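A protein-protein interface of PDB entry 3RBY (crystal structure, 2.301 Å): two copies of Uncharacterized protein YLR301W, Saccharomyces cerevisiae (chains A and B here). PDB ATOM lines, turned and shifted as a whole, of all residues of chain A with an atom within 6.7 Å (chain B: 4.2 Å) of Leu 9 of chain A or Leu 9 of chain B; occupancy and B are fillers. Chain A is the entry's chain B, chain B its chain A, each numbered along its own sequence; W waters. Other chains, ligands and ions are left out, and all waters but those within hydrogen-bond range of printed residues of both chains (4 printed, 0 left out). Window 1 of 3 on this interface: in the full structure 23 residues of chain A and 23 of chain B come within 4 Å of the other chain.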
ATOM      1  N   LYS A   7      33.718  -2.068  -4.280  1.00  0.00           N
ATOM      2  CA  LYS A   7      32.934  -3.098  -3.623  1.00  0.00           C
ATOM      3  C   LYS A   7      31.496  -3.016  -4.125  1.00  0.00           C
ATOM      4  O   LYS A   7      30.872  -1.947  -4.084  1.00  0.00           O
ATOM      5  CB  LYS A   7      33.008  -2.938  -2.109  1.00  0.00           C
ATOM      6  CG  LYS A   7      32.560  -4.186  -1.319  1.00  0.00           C
ATOM      7  CD  LYS A   7      31.051  -4.154  -1.056  1.00  0.00           C
ATOM      8  CE  LYS A   7      30.587  -5.314  -0.188  1.00  0.00           C
ATOM      9  NZ  LYS A   7      29.092  -5.319  -0.143  1.00  0.00           N
ATOM     10  N   ARG A   8      30.973  -4.132  -4.620  1.00  0.00           N
ATOM     11  CA  ARG A   8      29.611  -4.127  -5.145  1.00  0.00           C
ATOM     12  C   ARG A   8      28.571  -4.064  -4.031  1.00  0.00           C
ATOM     13  O   ARG A   8      28.641  -4.807  -3.038  1.00  0.00           O
ATOM     14  CB  ARG A   8      29.345  -5.324  -6.059  1.00  0.00           C
ATOM     15  CG  ARG A   8      28.243  -5.020  -7.070  1.00  0.00           C
ATOM     16  CD  ARG A   8      28.023  -6.156  -8.040  1.00  0.00           C
ATOM     17  NE  ARG A   8      27.392  -7.308  -7.396  1.00  0.00           N
ATOM     18  CZ  ARG A   8      27.162  -8.467  -8.009  1.00  0.00           C
ATOM     19  NH1 ARG A   8      27.530  -8.623  -9.277  1.00  0.00           N
ATOM     20  NH2 ARG A   8      26.576  -9.472  -7.353  1.00  0.00           N
ATOM     21  N   LEU A   9      27.613  -3.160  -4.210  1.00  0.00           N
ATOM     22  CA  LEU A   9      26.561  -2.921  -3.232  1.00  0.00           C
ATOM     23  C   LEU A   9      25.286  -3.655  -3.614  1.00  0.00           C
ATOM     24  O   LEU A   9      24.647  -4.271  -2.761  1.00  0.00           O
ATOM     25  CB  LEU A   9      26.272  -1.417  -3.143  1.00  0.00           C
ATOM     26  CG  LEU A   9      27.446  -0.540  -2.735  1.00  0.00           C
ATOM     27  CD1 LEU A   9      27.048   0.940  -2.764  1.00  0.00           C
ATOM     28  CD2 LEU A   9      27.967  -0.955  -1.353  1.00  0.00           C
ATOM     29  N   LEU A  10      24.901  -3.570  -4.891  1.00  0.00           N
ATOM     30  CA  LEU A  10      23.743  -4.322  -5.377  1.00  0.00           C
ATOM     31  C   LEU A  10      23.832  -4.726  -6.840  1.00  0.00           C
ATOM     32  O   LEU A  10      24.599  -4.154  -7.621  1.00  0.00           O
ATOM     33  CB  LEU A  10      22.417  -3.597  -5.092  1.00  0.00           C
ATOM     34  CG  LEU A  10      21.946  -2.353  -5.850  1.00  0.00           C
ATOM     35  CD1 LEU A  10      21.678  -2.637  -7.327  1.00  0.00           C
ATOM     36  CD2 LEU A  10      20.678  -1.832  -5.181  1.00  0.00           C
ATOM     37  N   PHE A  11      23.028  -5.728  -7.187  1.00  0.00           N
ATOM     38  CA  PHE A  11      22.994  -6.304  -8.530  1.00  0.00           C
ATOM     39  C   PHE A  11      21.541  -6.618  -8.890  1.00  0.00           C
ATOM     40  O   PHE A  11      20.887  -7.471  -8.266  1.00  0.00           O
ATOM     41  CB  PHE A  11      23.855  -7.567  -8.560  1.00  0.00           C
ATOM     42  CG  PHE A  11      23.827  -8.302  -9.871  1.00  0.00           C
ATOM     43  CD1 PHE A  11      23.806  -7.616 -11.074  1.00  0.00           C
ATOM     44  CD2 PHE A  11      23.864  -9.693  -9.897  1.00  0.00           C
ATOM     45  CE1 PHE A  11      23.799  -8.306 -12.280  1.00  0.00           C
ATOM     46  CE2 PHE A  11      23.857 -10.386 -11.096  1.00  0.00           C
ATOM     47  CZ  PHE A  11      23.823  -9.691 -12.290  1.00  0.00           C
ATOM     48  N   ASN A  18      19.362  -7.266  -5.301  1.00  0.00           N
ATOM     49  CA  ASN A  18      19.822  -8.080  -4.183  1.00  0.00           C
ATOM     50  C   ASN A  18      21.351  -8.102  -4.210  1.00  0.00           C
ATOM     51  O   ASN A  18      21.960  -7.562  -5.131  1.00  0.00           O
ATOM     52  CB  ASN A  18      19.238  -9.488  -4.313  1.00  0.00           C
ATOM     53  CG  ASN A  18      19.472 -10.359  -3.077  1.00  0.00           C
ATOM     54  OD1 ASN A  18      19.783  -9.868  -1.986  1.00  0.00           O
ATOM     55  ND2 ASN A  18      19.315 -11.673  -3.255  1.00  0.00           N
ATOM     56  N   GLU A  19      21.983  -8.708  -3.211  1.00  0.00           N
ATOM     57  CA  GLU A  19      23.442  -8.826  -3.229  1.00  0.00           C
ATOM     58  C   GLU A  19      23.920 -10.063  -2.476  1.00  0.00           C
ATOM     59  O   GLU A  19      24.009 -10.078  -1.241  1.00  0.00           O
ATOM     60  CB  GLU A  19      24.132  -7.555  -2.705  1.00  0.00           C
ATOM     61  CG  GLU A  19      25.649  -7.621  -2.784  1.00  0.00           C
ATOM     62  CD  GLU A  19      26.136  -7.897  -4.205  1.00  0.00           C
ATOM     63  OE1 GLU A  19      26.323  -9.087  -4.562  1.00  0.00           O
ATOM     64  OE2 GLU A  19      26.318  -6.914  -4.966  1.00  0.00           O
ATOM     65  N   THR A  23      31.722  -9.009  -3.616  1.00  0.00           N
ATOM     66  CA  THR A  23      32.404  -8.699  -4.863  1.00  0.00           C
ATOM     67  C   THR A  23      33.312  -7.482  -4.741  1.00  0.00           C
ATOM     68  O   THR A  23      32.873  -6.397  -4.336  1.00  0.00           O
ATOM     69  CB  THR A  23      31.407  -8.446  -5.988  1.00  0.00           C
ATOM     70  OG1 THR A  23      30.823  -9.693  -6.363  1.00  0.00           O
ATOM     71  CG2 THR A  23      32.102  -7.813  -7.188  1.00  0.00           C
ATOM     72  N   TRP A 103      27.815   9.250  -8.945  1.00  0.00           N
ATOM     73  CA  TRP A 103      26.782   9.962  -8.200  1.00  0.00           C
ATOM     74  C   TRP A 103      27.460  10.976  -7.301  1.00  0.00           C
ATOM     75  O   TRP A 103      28.668  10.887  -7.066  1.00  0.00           O
ATOM     76  CB  TRP A 103      25.964   8.984  -7.359  1.00  0.00           C
ATOM     77  CG  TRP A 103      25.036   8.115  -8.162  1.00  0.00           C
ATOM     78  CD1 TRP A 103      24.894   8.097  -9.517  1.00  0.00           C
ATOM     79  CD2 TRP A 103      24.106   7.140  -7.647  1.00  0.00           C
ATOM     80  NE1 TRP A 103      23.940   7.171  -9.883  1.00  0.00           N
ATOM     81  CE2 TRP A 103      23.441   6.572  -8.756  1.00  0.00           C
ATOM     82  CE3 TRP A 103      23.776   6.694  -6.355  1.00  0.00           C
ATOM     83  CZ2 TRP A 103      22.458   5.572  -8.616  1.00  0.00           C
ATOM     84  CZ3 TRP A 103      22.800   5.702  -6.216  1.00  0.00           C
ATOM     85  CH2 TRP A 103      22.151   5.157  -7.340  1.00  0.00           C
ATOM     86  N   SER A 105      27.217  11.091  -4.224  1.00  0.00           N
ATOM     87  CA  SER A 105      27.600  10.399  -2.997  1.00  0.00           C
ATOM     88  C   SER A 105      28.964   9.726  -3.149  1.00  0.00           C
ATOM     89  O   SER A 105      29.545   9.238  -2.168  1.00  0.00           O
ATOM     90  CB  SER A 105      26.551   9.352  -2.612  1.00  0.00           C
ATOM     91  OG  SER A 105      26.458   8.339  -3.598  1.00  0.00           O
ATOM     92  N   CYS A 107      29.503   7.029  -5.013  1.00  0.00           N
ATOM     93  CA  CYS A 107      29.332   5.681  -5.525  1.00  0.00           C
ATOM     94  C   CYS A 107      29.170   5.757  -7.036  1.00  0.00           C
ATOM     95  O   CYS A 107      28.882   6.835  -7.578  1.00  0.00           O
ATOM     96  CB  CYS A 107      28.107   5.012  -4.907  1.00  0.00           C
ATOM     97  SG  CYS A 107      28.354   4.467  -3.195  1.00  0.00           S
ATOM     98  N   VAL A 108      29.350   4.623  -7.717  1.00  0.00           N
ATOM     99  CA  VAL A 108      29.219   4.601  -9.173  1.00  0.00           C
ATOM    100  C   VAL A 108      28.169   3.605  -9.638  1.00  0.00           C
ATOM    101  O   VAL A 108      28.090   2.478  -9.132  1.00  0.00           O
ATOM    102  CB  VAL A 108      30.563   4.329  -9.880  1.00  0.00           C
ATOM    103  CG1 VAL A 108      30.421   4.586 -11.393  1.00  0.00           C
ATOM    104  CG2 VAL A 108      31.650   5.220  -9.294  1.00  0.00           C
ATOM    105  N   GLU A 128      24.322  -2.401 -11.684  1.00  0.00           N
ATOM    106  CA  GLU A 128      25.131  -2.734 -10.509  1.00  0.00           C
ATOM    107  C   GLU A 128      25.627  -1.470  -9.818  1.00  0.00           C
ATOM    108  O   GLU A 128      26.026  -0.511 -10.487  1.00  0.00           O
ATOM    109  CB  GLU A 128      26.305  -3.627 -10.898  1.00  0.00           C
ATOM    110  CG  GLU A 128      25.860  -4.951 -11.452  1.00  0.00           C
ATOM    111  CD  GLU A 128      26.979  -5.704 -12.133  1.00  0.00           C
ATOM    112  OE1 GLU A 128      27.115  -5.601 -13.380  1.00  0.00           O
ATOM    113  OE2 GLU A 128      27.718  -6.407 -11.413  1.00  0.00           O
ATOM    114  N   MET A 129      25.599  -1.458  -8.485  1.00  0.00           N
ATOM    115  CA  MET A 129      26.046  -0.279  -7.754  1.00  0.00           C
ATOM    116  C   MET A 129      27.378  -0.534  -7.080  1.00  0.00           C
ATOM    117  O   MET A 129      27.572  -1.548  -6.410  1.00  0.00           O
ATOM    118  CB  MET A 129      25.007   0.173  -6.735  1.00  0.00           C
ATOM    119  CG  MET A 129      23.719   0.715  -7.357  1.00  0.00           C
ATOM    120  SD  MET A 129      23.892   2.189  -8.415  1.00  0.00           S
ATOM    121  CE  MET A 129      24.853   3.279  -7.346  1.00  0.00           C
ATOM    122  N   TRP A 130      28.301   0.402  -7.260  1.00  0.00           N
ATOM    123  CA  TRP A 130      29.662   0.223  -6.777  1.00  0.00           C
ATOM    124  C   TRP A 130      30.058   1.269  -5.761  1.00  0.00           C
ATOM    125  O   TRP A 130      29.758   2.464  -5.925  1.00  0.00           O
ATOM    126  CB  TRP A 130      30.642   0.269  -7.950  1.00  0.00           C
ATOM    127  CG  TRP A 130      30.407  -0.856  -8.904  1.00  0.00           C
ATOM    128  CD1 TRP A 130      29.642  -0.829 -10.045  1.00  0.00           C
ATOM    129  CD2 TRP A 130      30.909  -2.191  -8.786  1.00  0.00           C
ATOM    130  NE1 TRP A 130      29.653  -2.069 -10.649  1.00  0.00           N
ATOM    131  CE2 TRP A 130      30.421  -2.925  -9.898  1.00  0.00           C
ATOM    132  CE3 TRP A 130      31.734  -2.840  -7.855  1.00  0.00           C
ATOM    133  CZ2 TRP A 130      30.732  -4.282 -10.102  1.00  0.00           C
ATOM    134  CZ3 TRP A 130      32.035  -4.194  -8.050  1.00  0.00           C
ATOM    135  CH2 TRP A 130      31.539  -4.896  -9.172  1.00  0.00           C
ATOM    136  N   GLN A 131      30.752   0.796  -4.728  1.00  0.00           N
ATOM    137  CA  GLN A 131      31.313   1.638  -3.696  1.00  0.00           C
ATOM    138  C   GLN A 131      32.825   1.619  -3.796  1.00  0.00           C
ATOM    139  O   GLN A 131      33.436   0.597  -3.507  1.00  0.00           O
ATOM    140  CB  GLN A 131      30.949   1.085  -2.318  1.00  0.00           C
ATOM    141  CG  GLN A 131      31.557   1.906  -1.190  1.00  0.00           C
ATOM    142  CD  GLN A 131      31.020   3.326  -1.203  1.00  0.00           C
ATOM    143  OE1 GLN A 131      29.856   3.556  -0.843  1.00  0.00           O
ATOM    144  NE2 GLN A 131      31.853   4.290  -1.644  1.00  0.00           N
ATOM    145  N   ILE A 142      34.984   3.442   3.171  1.00  0.00           N
ATOM    146  CA  ILE A 142      34.343   4.219   2.121  1.00  0.00           C
ATOM    147  C   ILE A 142      35.161   5.481   1.780  1.00  0.00           C
ATOM    148  O   ILE A 142      35.669   6.173   2.679  1.00  0.00           O
ATOM    149  CB  ILE A 142      32.896   4.571   2.546  1.00  0.00           C
ATOM    150  CG1 ILE A 142      32.053   3.291   2.580  1.00  0.00           C
ATOM    151  CG2 ILE A 142      32.272   5.595   1.612  1.00  0.00           C
ATOM    152  CD1 ILE A 142      30.673   3.464   3.208  1.00  0.00           C
ATOM    153  N   LYS B   7      24.607   4.301   6.830  1.00  0.00           N
ATOM    154  CA  LYS B   7      24.890   5.281   5.793  1.00  0.00           C
ATOM    155  C   LYS B   7      24.005   4.939   4.599  1.00  0.00           C
ATOM    156  O   LYS B   7      23.990   3.781   4.151  1.00  0.00           O
ATOM    157  CB  LYS B   7      26.360   5.209   5.407  1.00  0.00           C
ATOM    158  CG  LYS B   7      26.855   6.381   4.577  1.00  0.00           C
ATOM    159  CD  LYS B   7      26.679   6.146   3.076  1.00  0.00           C
ATOM    160  CE  LYS B   7      26.897   7.465   2.307  1.00  0.00           C
ATOM    161  NZ  LYS B   7      26.719   7.319   0.828  1.00  0.00           N
ATOM    162  N   ARG B   8      23.226   5.902   4.108  1.00  0.00           N
ATOM    163  CA  ARG B   8      22.353   5.587   2.983  1.00  0.00           C
ATOM    164  C   ARG B   8      23.165   5.526   1.692  1.00  0.00           C
ATOM    165  O   ARG B   8      24.006   6.395   1.449  1.00  0.00           O
ATOM    166  CB  ARG B   8      21.191   6.575   2.846  1.00  0.00           C
ATOM    167  CG  ARG B   8      20.210   6.121   1.784  1.00  0.00           C
ATOM    168  CD  ARG B   8      18.812   6.687   1.942  1.00  0.00           C
ATOM    169  NE  ARG B   8      18.740   8.140   1.780  1.00  0.00           N
ATOM    170  CZ  ARG B   8      18.803   8.761   0.614  1.00  0.00           C
ATOM    171  NH1 ARG B   8      18.974   8.044  -0.487  1.00  0.00           N
ATOM    172  NH2 ARG B   8      18.721  10.087   0.534  1.00  0.00           N
ATOM    173  N   LEU B   9      22.902   4.491   0.887  1.00  0.00           N
ATOM    174  CA  LEU B   9      23.628   4.214  -0.360  1.00  0.00           C
ATOM    175  C   LEU B   9      22.838   4.636  -1.590  1.00  0.00           C
ATOM    176  O   LEU B   9      23.425   4.992  -2.613  1.00  0.00           O
ATOM    177  CB  LEU B   9      23.940   2.721  -0.484  1.00  0.00           C
ATOM    178  CG  LEU B   9      24.851   2.146   0.596  1.00  0.00           C
ATOM    179  CD1 LEU B   9      24.923   0.611   0.490  1.00  0.00           C
ATOM    180  CD2 LEU B   9      26.237   2.789   0.510  1.00  0.00           C
ATOM    181  N   LEU B  10      21.512   4.555  -1.502  1.00  0.00           N
ATOM    182  CA  LEU B  10      20.658   5.042  -2.577  1.00  0.00           C
ATOM    183  C   LEU B  10      19.234   5.246  -2.114  1.00  0.00           C
ATOM    184  O   LEU B  10      18.779   4.597  -1.167  1.00  0.00           O
ATOM    185  CB  LEU B  10      20.689   4.113  -3.803  1.00  0.00           C
ATOM    186  CG  LEU B  10      19.855   2.835  -3.801  1.00  0.00           C
ATOM    187  CD1 LEU B  10      18.382   3.125  -4.128  1.00  0.00           C
ATOM    188  CD2 LEU B  10      20.427   1.854  -4.811  1.00  0.00           C
ATOM    189  N   GLU B  19      21.720   9.074  -5.417  1.00  0.00           N
ATOM    190  CA  GLU B  19      22.010   9.408  -4.030  1.00  0.00           C
ATOM    191  C   GLU B  19      22.608  10.807  -3.982  1.00  0.00           C
ATOM    192  O   GLU B  19      23.807  10.980  -4.233  1.00  0.00           O
ATOM    193  CB  GLU B  19      22.942   8.369  -3.372  1.00  0.00           C
ATOM    194  CG  GLU B  19      23.305   8.677  -1.920  1.00  0.00           C
ATOM    195  CD  GLU B  19      22.063   8.868  -1.055  1.00  0.00           C
ATOM    196  OE1 GLU B  19      21.500   7.849  -0.591  1.00  0.00           O
ATOM    197  OE2 GLU B  19      21.636  10.031  -0.867  1.00  0.00           O
ATOM    198  N   TRP B 103      20.267  -8.166   3.617  1.00  0.00           N
ATOM    199  CA  TRP B 103      20.827  -8.966   2.520  1.00  0.00           C
ATOM    200  C   TRP B 103      22.048  -9.730   2.991  1.00  0.00           C
ATOM    201  O   TRP B 103      22.643  -9.382   4.014  1.00  0.00           O
ATOM    202  CB  TRP B 103      21.221  -8.087   1.342  1.00  0.00           C
ATOM    203  CG  TRP B 103      20.073  -7.507   0.628  1.00  0.00           C
ATOM    204  CD1 TRP B 103      18.757  -7.715   0.897  1.00  0.00           C
ATOM    205  CD2 TRP B 103      20.121  -6.596  -0.485  1.00  0.00           C
ATOM    206  NE1 TRP B 103      17.976  -6.996   0.018  1.00  0.00           N
ATOM    207  CE2 TRP B 103      18.790  -6.301  -0.840  1.00  0.00           C
ATOM    208  CE3 TRP B 103      21.161  -6.004  -1.213  1.00  0.00           C
ATOM    209  CZ2 TRP B 103      18.469  -5.435  -1.894  1.00  0.00           C
ATOM    210  CZ3 TRP B 103      20.841  -5.150  -2.263  1.00  0.00           C
ATOM    211  CH2 TRP B 103      19.507  -4.874  -2.592  1.00  0.00           C
ATOM    212  N   CYS B 107      24.240  -5.339   3.948  1.00  0.00           N
ATOM    213  CA  CYS B 107      23.418  -4.140   3.764  1.00  0.00           C
ATOM    214  C   CYS B 107      21.956  -4.463   4.032  1.00  0.00           C
ATOM    215  O   CYS B 107      21.593  -5.638   4.204  1.00  0.00           O
ATOM    216  CB  CYS B 107      23.542  -3.599   2.334  1.00  0.00           C
ATOM    217  SG  CYS B 107      25.086  -2.739   2.050  1.00  0.00           S
ATOM    218  N   MET B 129      18.583   1.851   0.175  1.00  0.00           N
ATOM    219  CA  MET B 129      19.590   0.872   0.537  1.00  0.00           C
ATOM    220  C   MET B 129      20.502   1.444   1.610  1.00  0.00           C
ATOM    221  O   MET B 129      20.968   2.589   1.500  1.00  0.00           O
ATOM    222  CB  MET B 129      20.382   0.462  -0.696  1.00  0.00           C
ATOM    223  CG  MET B 129      20.534  -1.044  -0.863  1.00  0.00           C
ATOM    224  SD  MET B 129      18.946  -1.881  -0.904  1.00  0.00           S
ATOM    225  CE  MET B 129      18.109  -0.782  -2.001  1.00  0.00           C
ATOM    226  N   GLN B 131      23.833   0.967   4.381  1.00  0.00           N
ATOM    227  CA  GLN B 131      25.086   0.353   4.754  1.00  0.00           C
ATOM    228  C   GLN B 131      25.364   0.537   6.257  1.00  0.00           C
ATOM    229  O   GLN B 131      25.602   1.657   6.721  1.00  0.00           O
ATOM    230  CB  GLN B 131      26.232   0.967   3.947  1.00  0.00           C
ATOM    231  CG  GLN B 131      27.590   0.431   4.382  1.00  0.00           C
ATOM    232  CD  GLN B 131      27.771  -1.026   4.000  1.00  0.00           C
ATOM    233  OE1 GLN B 131      27.924  -1.343   2.811  1.00  0.00           O
ATOM    234  NE2 GLN B 131      27.738  -1.925   4.993  1.00  0.00           N
HETATM  235  O   HOH W   1      29.234   5.976   0.124  1.00  0.00           O
HETATM  236  O   HOH W   2      25.848   6.062  -2.209  1.00  0.00           O
HETATM  237  O   HOH W   3      25.553  -4.656  -0.383  1.00  0.00           O
HETATM  238  O   HOH W   4      28.906  -3.853   2.164  1.00  0.00           O
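O of Glu 19 of chain B lies within hydrogen-bond range of N of Ser 105 of chain A (3.4 Å).
The backbone NH of Lys 7 of chain B sits at hydrogen-bond distance from the backbone carbonyl oxygen of Gln 131 of chain B (2.8 Å). The backbone NH of Leu 9 of chain B sits at hydrogen-bond distance from the backbone carbonyl oxygen of Met 129 of chain B, 2.8 Å away. NE of Arg 8 of chain A lies within salt-bridge range of OE2 of Glu 19 of chain A (2.7 Å). N of Leu 9 of chain A lies within hydrogen-bond range of O of Met 129 of chain A. The backbone carbonyl oxygen (O) of Leu 10 of chain A is in hydrogen-bond range of the backbone NH (N) of Met 129 of chain A. The side-chain amide oxygen (OE1) of Gln 131 of chain A sits at hydrogen-bond distance from the side-chain sulfur (SG) of Cys 107 of chain A (2.9 Å).
Among the printed residues, pairs that only touch across the chains: Leu 9 of chain A with Leu 9 of chain B, Leu 9 of chain A with Trp 103 of chain B, Leu 10 of chain A with Leu 10 of chain B, Leu 10 of chain A with Trp 103 of chain B, Asn 18 of chain A with Trp 103 of chain B, Glu 19 of chain A with Trp 103 of chain B, Trp 103 of chain A with Leu 9 of chain B, Trp 103 of chain A with Leu 10 of chain B, Trp 103 of chain A with Glu 19 of chain B, Ser 105 of chain A with Lys 7 of chain B and Gln 131 of chain A with Leu 9 of chain B.
Of chain B, only Leu 9 (3.8 Å) and Trp 103 (3.9 Å) come within 4 Å of Leu 9 of chain A. Of chain A, only Leu 9, Trp 103 and Gln 131 come within 4 Å of Leu 9 of chain B. Of the printed residues of chain A, Glu 19 of chain B touches Trp 103 and Ser 105. Printed residues of chain B within 4 Å of Ser 105 of chain A: Lys 7 and Glu 19. Of the printed residues of chain A, Leu 10 of chain B touches Leu 10 and Trp 103. Of the printed residues of chain A, Trp 103 of chain B touches Leu 9, Leu 10, Asn 18 and Glu 19. Printed residues of chain B within 4 Å of Asn 18 of chain A: Trp 103 (3.5 Å). Cys 107 of chain A touches none of the printed residues of chain B. Lys 7 of chain A touches none of the printed residues of chain B. The nearest residue of chain A that does not touch Leu 9 of chain B is Cys 107 of chain A (4.6 Å). The nearest printed residue of chain B that does not touch Leu 10 of chain A is Met 129 of chain B (4.2 Å).
Hydrophobic or aromatic side chains of chain A that line the printed part of chain B: Leu 9, Leu 10 and Trp 103. Of the 9 printed residues of chain B, 5 touch a printed residue of chain A.
Leu 9 of chain A touches its own counterpart, Leu 9 of chain B. Leu 10 of chain A touches its own counterpart, Leu 10 of chain B. Glu 19 of chain A touches Trp 103 of chain B, and with the chains exchanged Trp 103 of chain A touches Glu 19 of chain B. Gln 131 of chain A touches Leu 9 of chain B, but with the chains exchanged Leu 9 of chain A does not touch Gln 131 of chain B (4.2 Å).
Water W3 bridges the backbone carbonyl oxygen (O) of Leu 9 of chain A (2.6 Å) and the side-chain sulfur (SG) of Cys 107 of chain B (3.1 Å). Water W1 lies within hydrogen-bond range of OE1 of Gln 131 of chain A (2.7 Å), NZ of Lys 7 of chain B (2.9 Å) and SG of Cys 107 of chain A (3.8 Å). Water W2 lies within hydrogen-bond range of O of Leu 9 of chain B (2.7 Å), OG of Ser 105 of chain A (2.7 Å), SG of Cys 107 of chain A (3.1 Å) and NZ of Lys 7 of chain B (3.4 Å). Water W4 bridges the side-chain amino group of Lys 7 of chain A (2.7 Å) and the side-chain amide oxygen of Gln 131 of chain B (2.8 Å).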
